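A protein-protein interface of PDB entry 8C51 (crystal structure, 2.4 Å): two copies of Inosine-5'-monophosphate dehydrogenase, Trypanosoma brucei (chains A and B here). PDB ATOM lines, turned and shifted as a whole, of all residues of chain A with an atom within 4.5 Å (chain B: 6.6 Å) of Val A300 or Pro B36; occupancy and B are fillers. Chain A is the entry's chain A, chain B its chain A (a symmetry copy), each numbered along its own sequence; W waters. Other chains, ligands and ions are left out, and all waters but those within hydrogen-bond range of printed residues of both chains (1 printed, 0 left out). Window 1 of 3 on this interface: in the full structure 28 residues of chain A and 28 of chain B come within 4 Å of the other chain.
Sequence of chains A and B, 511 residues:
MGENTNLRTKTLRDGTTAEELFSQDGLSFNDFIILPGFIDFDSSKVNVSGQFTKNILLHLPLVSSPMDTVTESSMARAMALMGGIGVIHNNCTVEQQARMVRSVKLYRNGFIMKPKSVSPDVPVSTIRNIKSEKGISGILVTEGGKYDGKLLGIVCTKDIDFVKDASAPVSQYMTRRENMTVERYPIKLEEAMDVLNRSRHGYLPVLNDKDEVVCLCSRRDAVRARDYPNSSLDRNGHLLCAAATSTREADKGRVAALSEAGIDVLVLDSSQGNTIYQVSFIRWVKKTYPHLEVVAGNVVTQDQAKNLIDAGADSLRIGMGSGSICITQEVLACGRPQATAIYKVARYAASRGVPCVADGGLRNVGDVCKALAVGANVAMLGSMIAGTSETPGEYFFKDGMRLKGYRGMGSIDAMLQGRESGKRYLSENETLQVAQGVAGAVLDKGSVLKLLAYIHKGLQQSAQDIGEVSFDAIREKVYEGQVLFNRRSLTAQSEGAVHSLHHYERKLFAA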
ATOM      1  N   GLN A 272     -31.145 -10.956   0.982  1.00  0.00           N
ATOM      2  CA  GLN A 272     -30.408 -10.060   0.094  1.00  0.00           C
ATOM      3  C   GLN A 272     -30.472 -10.678  -1.300  1.00  0.00           C
ATOM      4  O   GLN A 272     -29.677 -11.563  -1.631  1.00  0.00           O
ATOM      5  CB  GLN A 272     -28.973  -9.879   0.569  1.00  0.00           C
ATOM      6  CG  GLN A 272     -28.436  -8.478   0.390  1.00  0.00           C
ATOM      7  CD  GLN A 272     -27.938  -8.237  -1.015  1.00  0.00           C
ATOM      8  OE1 GLN A 272     -28.715  -8.236  -1.971  1.00  0.00           O
ATOM      9  NE2 GLN A 272     -26.632  -8.041  -1.154  1.00  0.00           N
ATOM     10  N   VAL A 299     -34.834  -6.590  -1.764  1.00  0.00           N
ATOM     11  CA  VAL A 299     -33.976  -5.467  -2.116  1.00  0.00           C
ATOM     12  C   VAL A 299     -34.410  -4.245  -1.322  1.00  0.00           C
ATOM     13  O   VAL A 299     -35.510  -4.196  -0.765  1.00  0.00           O
ATOM     14  CB  VAL A 299     -34.018  -5.161  -3.630  1.00  0.00           C
ATOM     15  CG1 VAL A 299     -33.512  -6.351  -4.420  1.00  0.00           C
ATOM     16  CG2 VAL A 299     -35.432  -4.798  -4.058  1.00  0.00           C
ATOM     17  N   VAL A 300     -33.520  -3.254  -1.261  1.00  0.00           N
ATOM     18  CA  VAL A 300     -33.843  -1.987  -0.611  1.00  0.00           C
ATOM     19  C   VAL A 300     -33.194  -0.802  -1.326  1.00  0.00           C
ATOM     20  O   VAL A 300     -33.482   0.353  -0.997  1.00  0.00           O
ATOM     21  CB  VAL A 300     -33.453  -2.009   0.882  1.00  0.00           C
ATOM     22  CG1 VAL A 300     -34.326  -3.007   1.646  1.00  0.00           C
ATOM     23  CG2 VAL A 300     -31.977  -2.334   1.057  1.00  0.00           C
ATOM     24  N   THR A 301     -32.313  -1.064  -2.294  1.00  0.00           N
ATOM     25  CA  THR A 301     -31.669  -0.004  -3.060  1.00  0.00           C
ATOM     26  C   THR A 301     -32.000  -0.120  -4.546  1.00  0.00           C
ATOM     27  O   THR A 301     -32.360  -1.190  -5.044  1.00  0.00           O
ATOM     28  CB  THR A 301     -30.143  -0.029  -2.889  1.00  0.00           C
ATOM     29  OG1 THR A 301     -29.586  -1.077  -3.692  1.00  0.00           O
ATOM     30  CG2 THR A 301     -29.769  -0.252  -1.433  1.00  0.00           C
ATOM     31  N   GLN A 304     -29.617  -3.193  -7.289  1.00  0.00           N
ATOM     32  CA  GLN A 304     -30.251  -4.419  -6.809  1.00  0.00           C
ATOM     33  C   GLN A 304     -31.548  -4.512  -7.598  1.00  0.00           C
ATOM     34  O   GLN A 304     -31.814  -5.503  -8.280  1.00  0.00           O
ATOM     35  CB  GLN A 304     -30.618  -4.438  -5.319  1.00  0.00           C
ATOM     36  CG  GLN A 304     -29.515  -4.416  -4.261  1.00  0.00           C
ATOM     37  CD  GLN A 304     -30.113  -4.531  -2.863  1.00  0.00           C
ATOM     38  OE1 GLN A 304     -30.802  -3.621  -2.397  1.00  0.00           O
ATOM     39  NE2 GLN A 304     -29.876  -5.659  -2.201  1.00  0.00           N
ATOM     40  N   GLY A 319     -37.517  -4.656   1.418  1.00  0.00           N
ATOM     41  CA  GLY A 319     -37.362  -4.782   2.851  1.00  0.00           C
ATOM     42  C   GLY A 319     -36.099  -5.511   3.250  1.00  0.00           C
ATOM     43  O   GLY A 319     -35.784  -6.577   2.713  1.00  0.00           O
ATOM     44  N   MET A 320     -35.365  -4.936   4.201  1.00  0.00           N
ATOM     45  CA  MET A 320     -34.181  -5.592   4.748  1.00  0.00           C
ATOM     46  C   MET A 320     -33.881  -4.913   6.084  1.00  0.00           C
ATOM     47  O   MET A 320     -33.278  -3.837   6.112  1.00  0.00           O
ATOM     48  CB  MET A 320     -33.005  -5.504   3.792  1.00  0.00           C
ATOM     49  CG  MET A 320     -31.745  -6.178   4.306  1.00  0.00           C
ATOM     50  SD  MET A 320     -30.294  -5.784   3.314  1.00  0.00           S
ATOM     51  CE  MET A 320     -29.209  -7.137   3.743  1.00  0.00           C
ATOM     52  N   CYS A 334     -26.245  -4.363   7.938  1.00  0.00           N
ATOM     53  CA  CYS A 334     -26.647  -4.066   6.572  1.00  0.00           C
ATOM     54  C   CYS A 334     -28.164  -4.097   6.446  1.00  0.00           C
ATOM     55  O   CYS A 334     -28.815  -5.047   6.893  1.00  0.00           O
ATOM     56  CB  CYS A 334     -26.009  -5.069   5.607  1.00  0.00           C
ATOM     57  SG  CYS A 334     -26.382  -4.780   3.869  1.00  0.00           S
ATOM     58  N   GLY A 335     -28.709  -3.050   5.835  1.00  0.00           N
ATOM     59  CA  GLY A 335     -30.144  -2.922   5.660  1.00  0.00           C
ATOM     60  C   GLY A 335     -30.479  -1.494   5.277  1.00  0.00           C
ATOM     61  O   GLY A 335     -29.623  -0.759   4.786  1.00  0.00           O
ATOM     62  N   ARG A 336     -31.731  -1.104   5.523  1.00  0.00           N
ATOM     63  CA  ARG A 336     -32.145   0.260   5.212  1.00  0.00           C
ATOM     64  C   ARG A 336     -33.492   0.600   5.841  1.00  0.00           C
ATOM     65  O   ARG A 336     -34.410  -0.230   5.823  1.00  0.00           O
ATOM     66  CB  ARG A 336     -32.215   0.455   3.694  1.00  0.00           C
ATOM     67  CG  ARG A 336     -32.449   1.895   3.272  1.00  0.00           C
ATOM     68  CD  ARG A 336     -32.503   2.039   1.762  1.00  0.00           C
ATOM     69  NE  ARG A 336     -32.057   3.358   1.330  1.00  0.00           N
ATOM     70  CZ  ARG A 336     -31.994   3.748   0.064  1.00  0.00           C
ATOM     71  NH1 ARG A 336     -32.333   2.939  -0.927  1.00  0.00           N
ATOM     72  NH2 ARG A 336     -31.580   4.981  -0.215  1.00  0.00           N
ATOM     73  N   ALA A 341     -36.504   3.059   1.733  1.00  0.00           N
ATOM     74  CA  ALA A 341     -36.288   1.965   0.797  1.00  0.00           C
ATOM     75  C   ALA A 341     -37.477   1.821  -0.140  1.00  0.00           C
ATOM     76  O   ALA A 341     -37.316   1.709  -1.362  1.00  0.00           O
ATOM     77  CB  ALA A 341     -36.043   0.664   1.561  1.00  0.00           C
ATOM     78  N   VAL A 345     -36.925   2.469  -4.179  1.00  0.00           N
ATOM     79  CA  VAL A 345     -36.988   1.306  -5.054  1.00  0.00           C
ATOM     80  C   VAL A 345     -38.268   1.333  -5.878  1.00  0.00           C
ATOM     81  O   VAL A 345     -38.258   0.999  -7.068  1.00  0.00           O
ATOM     82  CB  VAL A 345     -36.868   0.009  -4.233  1.00  0.00           C
ATOM     83  CG1 VAL A 345     -37.209  -1.196  -5.095  1.00  0.00           C
ATOM     84  CG2 VAL A 345     -35.466  -0.129  -3.657  1.00  0.00           C
ATOM     85  N   LYS B  10     -22.069  -0.026  -9.061  1.00  0.00           N
ATOM     86  CA  LYS B  10     -23.230   0.838  -8.904  1.00  0.00           C
ATOM     87  C   LYS B  10     -23.065   2.066  -9.789  1.00  0.00           C
ATOM     88  O   LYS B  10     -22.077   2.797  -9.664  1.00  0.00           O
ATOM     89  CB  LYS B  10     -23.402   1.259  -7.447  1.00  0.00           C
ATOM     90  CG  LYS B  10     -23.446   0.116  -6.446  1.00  0.00           C
ATOM     91  CD  LYS B  10     -23.722   0.646  -5.042  1.00  0.00           C
ATOM     92  CE  LYS B  10     -23.737  -0.461  -4.001  1.00  0.00           C
ATOM     93  NZ  LYS B  10     -22.602  -1.415  -4.162  1.00  0.00           N
ATOM     94  N   ASP B  14     -27.673   4.666  -5.520  1.00  0.00           N
ATOM     95  CA  ASP B  14     -28.777   5.003  -4.624  1.00  0.00           C
ATOM     96  C   ASP B  14     -28.308   4.799  -3.190  1.00  0.00           C
ATOM     97  O   ASP B  14     -28.282   3.675  -2.683  1.00  0.00           O
ATOM     98  CB  ASP B  14     -30.001   4.149  -4.933  1.00  0.00           C
ATOM     99  CG  ASP B  14     -31.099   4.306  -3.897  1.00  0.00           C
ATOM    100  OD1 ASP B  14     -31.174   5.379  -3.262  1.00  0.00           O
ATOM    101  OD2 ASP B  14     -31.892   3.357  -3.722  1.00  0.00           O
ATOM    102  N   ILE B  34     -25.284   0.270   6.629  1.00  0.00           N
ATOM    103  CA  ILE B  34     -24.625   0.058   5.348  1.00  0.00           C
ATOM    104  C   ILE B  34     -25.624  -0.560   4.383  1.00  0.00           C
ATOM    105  O   ILE B  34     -26.339  -1.507   4.732  1.00  0.00           O
ATOM    106  CB  ILE B  34     -23.386  -0.840   5.500  1.00  0.00           C
ATOM    107  CG1 ILE B  34     -22.472  -0.312   6.606  1.00  0.00           C
ATOM    108  CG2 ILE B  34     -22.633  -0.918   4.176  1.00  0.00           C
ATOM    109  CD1 ILE B  34     -21.322  -1.234   6.927  1.00  0.00           C
ATOM    110  N   LEU B  35     -25.671  -0.033   3.174  1.00  0.00           N
ATOM    111  CA  LEU B  35     -26.585  -0.567   2.183  1.00  0.00           C
ATOM    112  C   LEU B  35     -25.973  -1.794   1.510  1.00  0.00           C
ATOM    113  O   LEU B  35     -24.749  -1.900   1.395  1.00  0.00           O
ATOM    114  CB  LEU B  35     -26.915   0.493   1.141  1.00  0.00           C
ATOM    115  CG  LEU B  35     -27.610   1.728   1.717  1.00  0.00           C
ATOM    116  CD1 LEU B  35     -27.690   2.834   0.683  1.00  0.00           C
ATOM    117  CD2 LEU B  35     -28.997   1.368   2.234  1.00  0.00           C
ATOM    118  N   PRO B  36     -26.802  -2.737   1.072  1.00  0.00           N
ATOM    119  CA  PRO B  36     -26.277  -3.948   0.435  1.00  0.00           C
ATOM    120  C   PRO B  36     -25.810  -3.693  -0.991  1.00  0.00           C
ATOM    121  O   PRO B  36     -26.167  -2.703  -1.633  1.00  0.00           O
ATOM    122  CB  PRO B  36     -27.472  -4.907   0.459  1.00  0.00           C
ATOM    123  CG  PRO B  36     -28.661  -4.020   0.453  1.00  0.00           C
ATOM    124  CD  PRO B  36     -28.270  -2.776   1.202  1.00  0.00           C
ATOM    125  N   GLY B  37     -24.982  -4.620  -1.471  1.00  0.00           N
ATOM    126  CA  GLY B  37     -24.447  -4.554  -2.814  1.00  0.00           C
ATOM    127  C   GLY B  37     -24.819  -5.773  -3.632  1.00  0.00           C
ATOM    128  O   GLY B  37     -25.993  -6.153  -3.689  1.00  0.00           O
ATOM    129  N   PHE B  38     -23.826  -6.401  -4.257  1.00  0.00           N
ATOM    130  CA  PHE B  38     -24.038  -7.545  -5.134  1.00  0.00           C
ATOM    131  C   PHE B  38     -23.226  -8.732  -4.633  1.00  0.00           C
ATOM    132  O   PHE B  38     -22.041  -8.589  -4.319  1.00  0.00           O
ATOM    133  CB  PHE B  38     -23.645  -7.203  -6.571  1.00  0.00           C
ATOM    134  CG  PHE B  38     -23.765  -8.357  -7.513  1.00  0.00           C
ATOM    135  CD1 PHE B  38     -24.997  -8.718  -8.028  1.00  0.00           C
ATOM    136  CD2 PHE B  38     -22.651  -9.092  -7.872  1.00  0.00           C
ATOM    137  CE1 PHE B  38     -25.115  -9.785  -8.890  1.00  0.00           C
ATOM    138  CE2 PHE B  38     -22.760 -10.159  -8.734  1.00  0.00           C
ATOM    139  CZ  PHE B  38     -23.995 -10.509  -9.244  1.00  0.00           C
ATOM    140  N   ASP B 465     -23.154  -9.674   2.597  1.00  0.00           N
ATOM    141  CA  ASP B 465     -24.345  -8.875   2.337  1.00  0.00           C
ATOM    142  C   ASP B 465     -23.983  -7.542   1.693  1.00  0.00           C
ATOM    143  O   ASP B 465     -24.728  -7.037   0.846  1.00  0.00           O
ATOM    144  CB  ASP B 465     -25.126  -8.644   3.632  1.00  0.00           C
ATOM    145  CG  ASP B 465     -26.128  -9.749   3.920  1.00  0.00           C
ATOM    146  OD1 ASP B 465     -26.553  -9.870   5.088  1.00  0.00           O
ATOM    147  OD2 ASP B 465     -26.495 -10.494   2.985  1.00  0.00           O
ATOM    148  N   ILE B 466     -22.833  -6.970   2.066  1.00  0.00           N
ATOM    149  CA  ILE B 466     -22.396  -5.717   1.466  1.00  0.00           C
ATOM    150  C   ILE B 466     -21.937  -5.910   0.027  1.00  0.00           C
ATOM    151  O   ILE B 466     -21.953  -4.954  -0.758  1.00  0.00           O
ATOM    152  CB  ILE B 466     -21.274  -5.084   2.309  1.00  0.00           C
ATOM    153  CG1 ILE B 466     -21.832  -4.599   3.648  1.00  0.00           C
ATOM    154  CG2 ILE B 466     -20.624  -3.928   1.560  1.00  0.00           C
ATOM    155  CD1 ILE B 466     -20.771  -4.361   4.693  1.00  0.00           C
ATOM    156  N   GLY B 467     -21.520  -7.115  -0.340  1.00  0.00           N
ATOM    157  CA  GLY B 467     -21.167  -7.417  -1.709  1.00  0.00           C
ATOM    158  C   GLY B 467     -19.696  -7.328  -2.041  1.00  0.00           C
ATOM    159  O   GLY B 467     -19.359  -7.152  -3.217  1.00  0.00           O
ATOM    160  N   LEU B 484     -22.153   2.223  -0.016  1.00  0.00           N
ATOM    161  CA  LEU B 484     -22.988   3.349   0.356  1.00  0.00           C
ATOM    162  C   LEU B 484     -23.689   3.074   1.676  1.00  0.00           C
ATOM    163  O   LEU B 484     -23.805   1.929   2.121  1.00  0.00           O
ATOM    164  CB  LEU B 484     -24.015   3.646  -0.744  1.00  0.00           C
ATOM    165  CG  LEU B 484     -23.371   3.915  -2.105  1.00  0.00           C
ATOM    166  CD1 LEU B 484     -24.413   4.063  -3.199  1.00  0.00           C
ATOM    167  CD2 LEU B 484     -22.498   5.155  -2.023  1.00  0.00           C
HETATM  168  O   HOH W   1     -26.745  -2.116  -4.082  1.00  0.00           O
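Printed residues of chain B within 4 Å of Val A300: Pro B36.
Pro B36 touches just these residues of chain A: Gln A272 (3.6 Å), Val A300 (3.7 Å), Thr A301 (3.9 Å), Gln A304 (3.3 Å), Met A320 (3.7 Å) and Cys A334 (3.5 Å).
Of the printed residues of chain B, Met A320 touches Pro B36 (3.7 Å).
Of the printed residues of chain A, Leu B35 touches Thr A301 (3.9 Å), Cys A334 (3.8 Å), Gly A335 (3.4 Å) and Arg A336 (3.6 Å).
Printed residues of chain B within 4 Å of Gly A335: Ile B34 (3.0 Å) and Leu B35 (3.4 Å).
Of the printed residues of chain B, Gln A272 touches Pro B36 (3.6 Å), Gly B37 (3.2 Å) and Asp B465 (2.9 Å).
Printed residues of chain A within 4 Å of Ile B34: Cys A334 and Gly A335.
Lys B10 touches none of the printed residues of chain A.
Water W1 bridges O of Pro B36 (2.6 Å) and OG1 of Thr A301 (3.1 Å).
The backbone carbonyl oxygen of Leu B484 lies within hydrogen-bond range of the backbone NH of Leu B35.
The backbone NH (N) of Gly B37 is in hydrogen-bond range of the backbone carbonyl oxygen (O) of Asp B465 (3.4 Å).
The backbone NH of Arg A336 is in hydrogen-bond range of the backbone carbonyl oxygen of Met A320 (3.2 Å).
The backbone NH (N) of Thr A301 sits at hydrogen-bond distance from the side-chain amide oxygen (OE1) of Gln A304, 3.0 Å away.
The backbone NH (N) of Gly B37 sits at hydrogen-bond distance from the backbone carbonyl oxygen (O) of Ile B466 (3.1 Å).
The backbone NH of Val A300 sits at hydrogen-bond distance from the side-chain amide oxygen of Gln A304, at 3.0 Å.
O of Ile B34 lies close to SG of Cys A334 (3.4 Å).
N of Pro B36 lies close to SG of Cys A334 (3.5 Å).
The side-chain amide nitrogen (NE2) of Gln A272 sits at hydrogen-bond distance from the backbone carbonyl oxygen (O) of Gly B37, at 3.2 Å.
O of Ile B34 sits at hydrogen-bond distance from N of Gly A335 (3.0 Å).
The side-chain amide nitrogen (NE2) of Gln A272 sits at hydrogen-bond distance from the backbone carbonyl oxygen (O) of Asp B465, 2.9 Å away.
NH1 of Arg A336 lies within salt-bridge range of OD2 of Asp B14, 2.9 Å away.
Gln A272 touches Pro B36 (NE2 to CB, 3.6 Å).
Pro B36 touches Val A300 (CD to CG2, 3.7 Å).
CB of Leu B35 touches CG2 of Thr A301 (3.9 Å).
Thr A301 touches Pro B36.
Pro B36 touches Gln A304.
Gly B37 touches Gln A304 (O to CG, 3.97 Å).
Pro B36 touches Met A320.
Leu B35 touches Cys A334.
CD2 of Leu B35 touches O of Gly A335, at 3.4 Å.
Arg A336 touches Leu B35 (CD to CD2, 3.6 Å).
Of the 11 printed residues of chain B, 6 touch a printed residue of chain A.
Hydrophobic or aromatic side chains of chain B that line the printed part of chain A: Leu B35 and Pro B36.
Of the 12 printed residues of chain A, 8 touch a printed residue of chain B.
Printed residues of chain A that touch a printed residue of chain B: Gln A272, Val A300, Thr A301, Gln A304, Met A320, Cys A334, Gly A335 and Arg A336.
Among the printed residues, Asp or Glu carboxylates within 4 Å of a Lys or Arg side-chain nitrogen of the other chain: Arg A336 with Asp B14.
No position is printed for both chains.
Of the 17 pairs that touch across the chains among the printed residues, none has its exchanged pair printed and touching as well.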
